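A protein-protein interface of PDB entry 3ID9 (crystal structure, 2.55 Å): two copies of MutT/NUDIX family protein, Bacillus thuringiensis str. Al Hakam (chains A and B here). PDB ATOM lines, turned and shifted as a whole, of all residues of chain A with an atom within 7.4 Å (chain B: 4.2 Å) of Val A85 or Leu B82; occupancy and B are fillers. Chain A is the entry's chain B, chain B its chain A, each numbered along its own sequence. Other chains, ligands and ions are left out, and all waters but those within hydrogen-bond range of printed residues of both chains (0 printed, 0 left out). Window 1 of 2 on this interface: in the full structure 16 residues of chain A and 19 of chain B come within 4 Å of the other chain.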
ATOM      1  N   LEU A  61      24.849  11.202   8.048  1.00  0.00           N
ATOM      2  CA  LEU A  61      25.346   9.833   8.044  1.00  0.00           C
ATOM      3  C   LEU A  61      24.453   8.997   7.131  1.00  0.00           C
ATOM      4  O   LEU A  61      24.932   8.148   6.384  1.00  0.00           O
ATOM      5  CB  LEU A  61      25.319   9.233   9.451  1.00  0.00           C
ATOM      6  CG  LEU A  61      26.141   9.941  10.523  1.00  0.00           C
ATOM      7  CD1 LEU A  61      26.043   9.150  11.812  1.00  0.00           C
ATOM      8  CD2 LEU A  61      27.581  10.073  10.080  1.00  0.00           C
ATOM      9  N   LEU A  82      21.327   2.056  14.624  1.00  0.00           N
ATOM     10  CA  LEU A  82      22.742   2.328  14.768  1.00  0.00           C
ATOM     11  C   LEU A  82      23.238   1.094  15.518  1.00  0.00           C
ATOM     12  O   LEU A  82      22.783   0.804  16.624  1.00  0.00           O
ATOM     13  CB  LEU A  82      22.916   3.579  15.621  1.00  0.00           C
ATOM     14  CG  LEU A  82      24.202   4.392  15.620  1.00  0.00           C
ATOM     15  CD1 LEU A  82      25.378   3.443  15.526  1.00  0.00           C
ATOM     16  CD2 LEU A  82      24.188   5.376  14.466  1.00  0.00           C
ATOM     17  N   LEU A  83      24.157   0.351  14.925  1.00  0.00           N
ATOM     18  CA  LEU A  83      24.638  -0.848  15.582  1.00  0.00           C
ATOM     19  C   LEU A  83      25.884  -0.655  16.429  1.00  0.00           C
ATOM     20  O   LEU A  83      25.980  -1.169  17.549  1.00  0.00           O
ATOM     21  CB  LEU A  83      24.928  -1.937  14.544  1.00  0.00           C
ATOM     22  CG  LEU A  83      25.592  -3.184  15.138  1.00  0.00           C
ATOM     23  CD1 LEU A  83      24.570  -3.935  15.983  1.00  0.00           C
ATOM     24  CD2 LEU A  83      26.132  -4.078  14.031  1.00  0.00           C
ATOM     25  N   TYR A  84      26.839   0.092  15.898  1.00  0.00           N
ATOM     26  CA  TYR A  84      28.094   0.245  16.590  1.00  0.00           C
ATOM     27  C   TYR A  84      28.780   1.544  16.212  1.00  0.00           C
ATOM     28  O   TYR A  84      28.804   1.934  15.042  1.00  0.00           O
ATOM     29  CB  TYR A  84      28.978  -0.947  16.218  1.00  0.00           C
ATOM     30  CG  TYR A  84      30.264  -1.079  16.979  1.00  0.00           C
ATOM     31  CD1 TYR A  84      30.290  -1.649  18.251  1.00  0.00           C
ATOM     32  CD2 TYR A  84      31.469  -0.674  16.412  1.00  0.00           C
ATOM     33  CE1 TYR A  84      31.492  -1.819  18.940  1.00  0.00           C
ATOM     34  CE2 TYR A  84      32.674  -0.837  17.088  1.00  0.00           C
ATOM     35  CZ  TYR A  84      32.680  -1.412  18.348  1.00  0.00           C
ATOM     36  OH  TYR A  84      33.881  -1.596  19.000  1.00  0.00           O
ATOM     37  N   VAL A  85      29.330   2.213  17.217  1.00  0.00           N
ATOM     38  CA  VAL A  85      30.038   3.461  17.011  1.00  0.00           C
ATOM     39  C   VAL A  85      31.429   3.269  17.590  1.00  0.00           C
ATOM     40  O   VAL A  85      31.595   2.863  18.741  1.00  0.00           O
ATOM     41  CB  VAL A  85      29.322   4.650  17.703  1.00  0.00           C
ATOM     42  CG1 VAL A  85      30.175   5.900  17.594  1.00  0.00           C
ATOM     43  CG2 VAL A  85      27.967   4.895  17.045  1.00  0.00           C
ATOM     44  N   CYS A  86      32.427   3.531  16.761  1.00  0.00           N
ATOM     45  CA  CYS A  86      33.810   3.381  17.167  1.00  0.00           C
ATOM     46  C   CYS A  86      34.526   4.696  16.898  1.00  0.00           C
ATOM     47  O   CYS A  86      34.499   5.204  15.776  1.00  0.00           O
ATOM     48  CB  CYS A  86      34.460   2.243  16.363  1.00  0.00           C
ATOM     49  SG  CYS A  86      36.245   2.054  16.628  1.00  0.00           S
ATOM     50  N   ASP A  87      35.140   5.274  17.925  1.00  0.00           N
ATOM     51  CA  ASP A  87      35.847   6.515  17.692  1.00  0.00           C
ATOM     52  C   ASP A  87      37.291   6.464  18.150  1.00  0.00           C
ATOM     53  O   ASP A  87      37.617   5.880  19.182  1.00  0.00           O
ATOM     54  CB  ASP A  87      35.081   7.721  18.283  1.00  0.00           C
ATOM     55  CG  ASP A  87      35.197   7.841  19.792  1.00  0.00           C
ATOM     56  OD1 ASP A  87      34.910   6.868  20.521  1.00  0.00           O
ATOM     57  OD2 ASP A  87      35.563   8.944  20.248  1.00  0.00           O
ATOM     58  N   LEU A  96      35.658   8.753  13.406  1.00  0.00           N
ATOM     59  CA  LEU A  96      34.412   8.276  13.967  1.00  0.00           C
ATOM     60  C   LEU A  96      33.878   7.265  12.943  1.00  0.00           C
ATOM     61  O   LEU A  96      33.697   7.590  11.769  1.00  0.00           O
ATOM     62  CB  LEU A  96      33.443   9.440  14.157  1.00  0.00           C
ATOM     63  CG  LEU A  96      32.152   9.104  14.901  1.00  0.00           C
ATOM     64  CD1 LEU A  96      32.479   8.561  16.283  1.00  0.00           C
ATOM     65  CD2 LEU A  96      31.292  10.344  15.006  1.00  0.00           C
ATOM     66  N   HIS A  97      33.661   6.031  13.382  1.00  0.00           N
ATOM     67  CA  HIS A  97      33.171   4.981  12.494  1.00  0.00           C
ATOM     68  C   HIS A  97      31.803   4.451  12.938  1.00  0.00           C
ATOM     69  O   HIS A  97      31.686   3.825  13.990  1.00  0.00           O
ATOM     70  CB  HIS A  97      34.182   3.827  12.453  1.00  0.00           C
ATOM     71  CG  HIS A  97      33.856   2.769  11.444  1.00  0.00           C
ATOM     72  ND1 HIS A  97      34.487   1.542  11.416  1.00  0.00           N
ATOM     73  CD2 HIS A  97      32.970   2.759  10.415  1.00  0.00           C
ATOM     74  CE1 HIS A  97      34.005   0.822  10.419  1.00  0.00           C
ATOM     75  NE2 HIS A  97      33.083   1.539   9.795  1.00  0.00           N
ATOM     76  N   ILE A  98      30.775   4.699  12.133  1.00  0.00           N
ATOM     77  CA  ILE A  98      29.425   4.235  12.451  1.00  0.00           C
ATOM     78  C   ILE A  98      28.979   3.042  11.589  1.00  0.00           C
ATOM     79  O   ILE A  98      29.127   3.059  10.367  1.00  0.00           O
ATOM     80  CB  ILE A  98      28.365   5.366  12.269  1.00  0.00           C
ATOM     81  CG1 ILE A  98      28.600   6.507  13.262  1.00  0.00           C
ATOM     82  CG2 ILE A  98      26.972   4.807  12.491  1.00  0.00           C
ATOM     83  CD1 ILE A  98      29.619   7.515  12.818  1.00  0.00           C
ATOM     84  N   THR A  99      28.423   2.020  12.238  1.00  0.00           N
ATOM     85  CA  THR A  99      27.926   0.833  11.550  1.00  0.00           C
ATOM     86  C   THR A  99      26.405   0.772  11.652  1.00  0.00           C
ATOM     87  O   THR A  99      25.847   0.778  12.753  1.00  0.00           O
ATOM     88  CB  THR A  99      28.508  -0.469  12.153  1.00  0.00           C
ATOM     89  OG1 THR A  99      29.883  -0.600  11.776  1.00  0.00           O
ATOM     90  CG2 THR A  99      27.744  -1.685  11.646  1.00  0.00           C
ATOM     91  N   LEU A 144      28.661  -9.751  17.360  1.00  0.00           N
ATOM     92  CA  LEU A 144      27.967  -8.472  17.326  1.00  0.00           C
ATOM     93  C   LEU A 144      26.868  -8.507  16.268  1.00  0.00           C
ATOM     94  O   LEU A 144      25.697  -8.268  16.556  1.00  0.00           O
ATOM     95  CB  LEU A 144      28.952  -7.350  17.003  1.00  0.00           C
ATOM     96  CG  LEU A 144      28.362  -5.945  16.933  1.00  0.00           C
ATOM     97  CD1 LEU A 144      28.067  -5.452  18.340  1.00  0.00           C
ATOM     98  CD2 LEU A 144      29.339  -5.016  16.244  1.00  0.00           C
ATOM     99  N   ALA A 152      22.169  -3.412  19.259  1.00  0.00           N
ATOM    100  CA  ALA A 152      22.079  -2.045  18.761  1.00  0.00           C
ATOM    101  C   ALA A 152      22.557  -1.061  19.838  1.00  0.00           C
ATOM    102  O   ALA A 152      22.419  -1.327  21.030  1.00  0.00           O
ATOM    103  CB  ALA A 152      20.642  -1.733  18.372  1.00  0.00           C
ATOM    104  N   GLY A 153      23.121   0.067  19.415  1.00  0.00           N
ATOM    105  CA  GLY A 153      23.591   1.062  20.363  1.00  0.00           C
ATOM    106  C   GLY A 153      24.903   0.747  21.072  1.00  0.00           C
ATOM    107  O   GLY A 153      25.164   1.282  22.152  1.00  0.00           O
ATOM    108  N   SER A 154      25.724  -0.121  20.484  1.00  0.00           N
ATOM    109  CA  SER A 154      27.010  -0.472  21.079  1.00  0.00           C
ATOM    110  C   SER A 154      28.020   0.632  20.794  1.00  0.00           C
ATOM    111  O   SER A 154      27.985   1.258  19.735  1.00  0.00           O
ATOM    112  CB  SER A 154      27.532  -1.792  20.507  1.00  0.00           C
ATOM    113  OG  SER A 154      26.733  -2.878  20.922  1.00  0.00           O
ATOM    114  N   TYR A 155      28.928   0.857  21.731  1.00  0.00           N
ATOM    115  CA  TYR A 155      29.926   1.900  21.563  1.00  0.00           C
ATOM    116  C   TYR A 155      31.281   1.517  22.135  1.00  0.00           C
ATOM    117  O   TYR A 155      31.379   0.721  23.065  1.00  0.00           O
ATOM    118  CB  TYR A 155      29.462   3.188  22.240  1.00  0.00           C
ATOM    119  CG  TYR A 155      30.586   4.177  22.440  1.00  0.00           C
ATOM    120  CD1 TYR A 155      31.005   5.016  21.406  1.00  0.00           C
ATOM    121  CD2 TYR A 155      31.286   4.221  23.645  1.00  0.00           C
ATOM    122  CE1 TYR A 155      32.093   5.868  21.568  1.00  0.00           C
ATOM    123  CE2 TYR A 155      32.377   5.068  23.814  1.00  0.00           C
ATOM    124  CZ  TYR A 155      32.775   5.888  22.776  1.00  0.00           C
ATOM    125  OH  TYR A 155      33.856   6.725  22.952  1.00  0.00           O
ATOM    126  N   GLN A 156      32.331   2.111  21.593  1.00  0.00           N
ATOM    127  CA  GLN A 156      33.664   1.830  22.075  1.00  0.00           C
ATOM    128  C   GLN A 156      34.593   2.965  21.696  1.00  0.00           C
ATOM    129  O   GLN A 156      34.599   3.410  20.550  1.00  0.00           O
ATOM    130  CB  GLN A 156      34.162   0.523  21.474  1.00  0.00           C
ATOM    131  CG  GLN A 156      35.501   0.065  21.997  1.00  0.00           C
ATOM    132  CD  GLN A 156      35.965  -1.220  21.324  1.00  0.00           C
ATOM    133  OE1 GLN A 156      35.247  -2.225  21.315  1.00  0.00           O
ATOM    134  NE2 GLN A 156      37.167  -1.194  20.758  1.00  0.00           N
ATOM    135  N   GLY A 157      35.353   3.450  22.673  1.00  0.00           N
ATOM    136  CA  GLY A 157      36.304   4.516  22.426  1.00  0.00           C
ATOM    137  C   GLY A 157      37.683   3.879  22.427  1.00  0.00           C
ATOM    138  O   GLY A 157      37.986   3.058  23.291  1.00  0.00           O
ATOM    139  N   LYS B  81      24.605   2.435  27.317  1.00  0.00           N
ATOM    140  CA  LYS B  81      24.374   2.209  25.903  1.00  0.00           C
ATOM    141  C   LYS B  81      24.280   3.519  25.163  1.00  0.00           C
ATOM    142  O   LYS B  81      24.080   4.569  25.762  1.00  0.00           O
ATOM    143  CB  LYS B  81      23.090   1.419  25.657  1.00  0.00           C
ATOM    144  CG  LYS B  81      23.314  -0.073  25.598  1.00  0.00           C
ATOM    145  CD  LYS B  81      22.315  -0.765  24.699  1.00  0.00           C
ATOM    146  CE  LYS B  81      22.538  -2.274  24.734  1.00  0.00           C
ATOM    147  NZ  LYS B  81      23.968  -2.623  24.479  1.00  0.00           N
ATOM    148  N   LEU B  82      24.442   3.451  23.850  1.00  0.00           N
ATOM    149  CA  LEU B  82      24.343   4.634  23.027  1.00  0.00           C
ATOM    150  C   LEU B  82      22.888   4.668  22.579  1.00  0.00           C
ATOM    151  O   LEU B  82      22.426   3.789  21.851  1.00  0.00           O
ATOM    152  CB  LEU B  82      25.297   4.534  21.835  1.00  0.00           C
ATOM    153  CG  LEU B  82      25.276   5.700  20.848  1.00  0.00           C
ATOM    154  CD1 LEU B  82      26.533   5.701  20.012  1.00  0.00           C
ATOM    155  CD2 LEU B  82      24.046   5.592  19.974  1.00  0.00           C
ATOM    156  N   LEU B  83      22.159   5.668  23.044  1.00  0.00           N
ATOM    157  CA  LEU B  83      20.757   5.796  22.699  1.00  0.00           C
ATOM    158  C   LEU B  83      20.563   7.043  21.886  1.00  0.00           C
ATOM    159  O   LEU B  83      20.731   8.142  22.400  1.00  0.00           O
ATOM    160  CB  LEU B  83      19.902   5.893  23.962  1.00  0.00           C
ATOM    161  CG  LEU B  83      18.416   6.139  23.681  1.00  0.00           C
ATOM    162  CD1 LEU B  83      17.583   5.015  24.278  1.00  0.00           C
ATOM    163  CD2 LEU B  83      18.001   7.489  24.239  1.00  0.00           C
ATOM    164  N   TYR B  84      20.216   6.890  20.618  1.00  0.00           N
ATOM    165  CA  TYR B  84      19.992   8.053  19.763  1.00  0.00           C
ATOM    166  C   TYR B  84      21.232   8.859  19.382  1.00  0.00           C
ATOM    167  O   TYR B  84      22.063   9.196  20.217  1.00  0.00           O
ATOM    168  CB  TYR B  84      18.990   9.007  20.412  1.00  0.00           C
ATOM    169  CG  TYR B  84      18.295   9.923  19.433  1.00  0.00           C
ATOM    170  CD1 TYR B  84      17.317   9.429  18.569  1.00  0.00           C
ATOM    171  CD2 TYR B  84      18.592  11.286  19.383  1.00  0.00           C
ATOM    172  CE1 TYR B  84      16.643  10.268  17.682  1.00  0.00           C
ATOM    173  CE2 TYR B  84      17.928  12.136  18.497  1.00  0.00           C
ATOM    174  CZ  TYR B  84      16.952  11.618  17.650  1.00  0.00           C
ATOM    175  OH  TYR B  84      16.276  12.443  16.776  1.00  0.00           O
ATOM    176  N   ILE B  98      25.295  13.052  20.116  1.00  0.00           N
ATOM    177  CA  ILE B  98      25.133  11.692  20.638  1.00  0.00           C
ATOM    178  C   ILE B  98      24.575  11.650  22.069  1.00  0.00           C
ATOM    179  O   ILE B  98      25.086  12.315  22.964  1.00  0.00           O
ATOM    180  CB  ILE B  98      26.480  10.911  20.634  1.00  0.00           C
ATOM    181  CG1 ILE B  98      27.053  10.835  19.223  1.00  0.00           C
ATOM    182  CG2 ILE B  98      26.275   9.505  21.163  1.00  0.00           C
ATOM    183  CD1 ILE B  98      27.920  12.005  18.872  1.00  0.00           C
ATOM    184  N   THR B  99      23.541  10.845  22.286  1.00  0.00           N
ATOM    185  CA  THR B  99      22.944  10.735  23.606  1.00  0.00           C
ATOM    186  C   THR B  99      23.223   9.361  24.194  1.00  0.00           C
ATOM    187  O   THR B  99      22.985   8.346  23.559  1.00  0.00           O
ATOM    188  CB  THR B  99      21.423  11.012  23.533  1.00  0.00           C
ATOM    189  OG1 THR B  99      21.220  12.356  23.065  1.00  0.00           O
ATOM    190  CG2 THR B  99      20.774  10.863  24.898  1.00  0.00           C
ATOM    191  N   PHE B 100      23.735   9.335  25.416  1.00  0.00           N
ATOM    192  CA  PHE B 100      24.083   8.083  26.073  1.00  0.00           C
ATOM    193  C   PHE B 100      23.199   7.741  27.265  1.00  0.00           C
ATOM    194  O   PHE B 100      22.793   8.620  28.017  1.00  0.00           O
ATOM    195  CB  PHE B 100      25.523   8.143  26.586  1.00  0.00           C
ATOM    196  CG  PHE B 100      26.567   8.012  25.528  1.00  0.00           C
ATOM    197  CD1 PHE B 100      26.768   6.797  24.872  1.00  0.00           C
ATOM    198  CD2 PHE B 100      27.401   9.081  25.228  1.00  0.00           C
ATOM    199  CE1 PHE B 100      27.789   6.649  23.936  1.00  0.00           C
ATOM    200  CE2 PHE B 100      28.426   8.946  24.293  1.00  0.00           C
ATOM    201  CZ  PHE B 100      28.620   7.725  23.647  1.00  0.00           C
ATOM    202  N   ALA B 152      17.703   1.745  21.996  1.00  0.00           N
ATOM    203  CA  ALA B 152      19.129   1.895  21.758  1.00  0.00           C
ATOM    204  C   ALA B 152      19.469   1.889  20.266  1.00  0.00           C
ATOM    205  O   ALA B 152      18.935   1.093  19.498  1.00  0.00           O
ATOM    206  CB  ALA B 152      19.887   0.778  22.470  1.00  0.00           C
ATOM    207  N   GLY B 153      20.357   2.787  19.861  1.00  0.00           N
ATOM    208  CA  GLY B 153      20.764   2.843  18.472  1.00  0.00           C
ATOM    209  C   GLY B 153      19.895   3.662  17.540  1.00  0.00           C
ATOM    210  O   GLY B 153      20.047   3.565  16.328  1.00  0.00           O
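The backbone carbonyl oxygen of Gly A153 lies within hydrogen-bond range of the backbone NH of Leu B82 (2.8 Å).
O of Gly B153 is in hydrogen-bond range of N of Leu A82, 2.6 Å away.
The backbone carbonyl oxygen (O) of Leu B82 is in hydrogen-bond range of the backbone NH (N) of Gly B153 (3.0 Å).
The backbone carbonyl oxygen (O) of Leu A82 is in hydrogen-bond range of the backbone NH (N) of Gly A153, 2.9 Å away.
O of Ser A154 sits at hydrogen-bond distance from N of Val A85 (3.0 Å).
The backbone carbonyl oxygen (O) of Val A85 is in hydrogen-bond range of the backbone NH (N) of Gln A156 (3.0 Å).
Val A85 touches Leu B82 (CG2 to CD1, 3.4 Å).
Lys B81 touches Ala A152 (CD to O, 3.7 Å).
O of Ala B152 touches CB of Ala A152, 3.5 Å away.
Gly A153 touches Lys B81 (O to C, 3.9 Å).
Gly B153 touches Gly A153.
Of chain B, only Leu B82 (3.4 Å) comes within 4 Å of Val A85.
Of chain A, only Val A85 (3.4 Å) and Gly A153 (2.8 Å) come within 4 Å of Leu B82.
Of the printed residues of chain A, Ala B152 touches Ala A152.
Printed residues of chain B within 4 Å of Leu A82: Gly B153 (2.6 Å).
Of the printed residues of chain A, Gly B153 touches Leu A82 and Gly A153.
Leu A61 touches none of the printed residues of chain B.
The nearest residue of chain A that does not touch Leu B82 is Tyr A155 (4.4 Å).
Printed residues of chain A that touch a printed residue of chain B: Leu A82, Val A85, Ala A152 and Gly A153.
Hydrophobic or aromatic side chains of chain A that line the printed part of chain B: Leu A82, Val A85 and Ala A152.
Along chain A the printed residues that touch a printed residue of chain B span positions 82 to 153.
Among the printed residues, no Asp or Glu carboxylate lies within 4 Å of a Lys or Arg side-chain nitrogen of the other chain.
Leu A82 touches Gly B153, and with the chains exchanged Gly A153 touches Leu B82.
Ala A152 touches its own counterpart, Ala B152.
Gly A153 touches its own counterpart, Gly B153.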
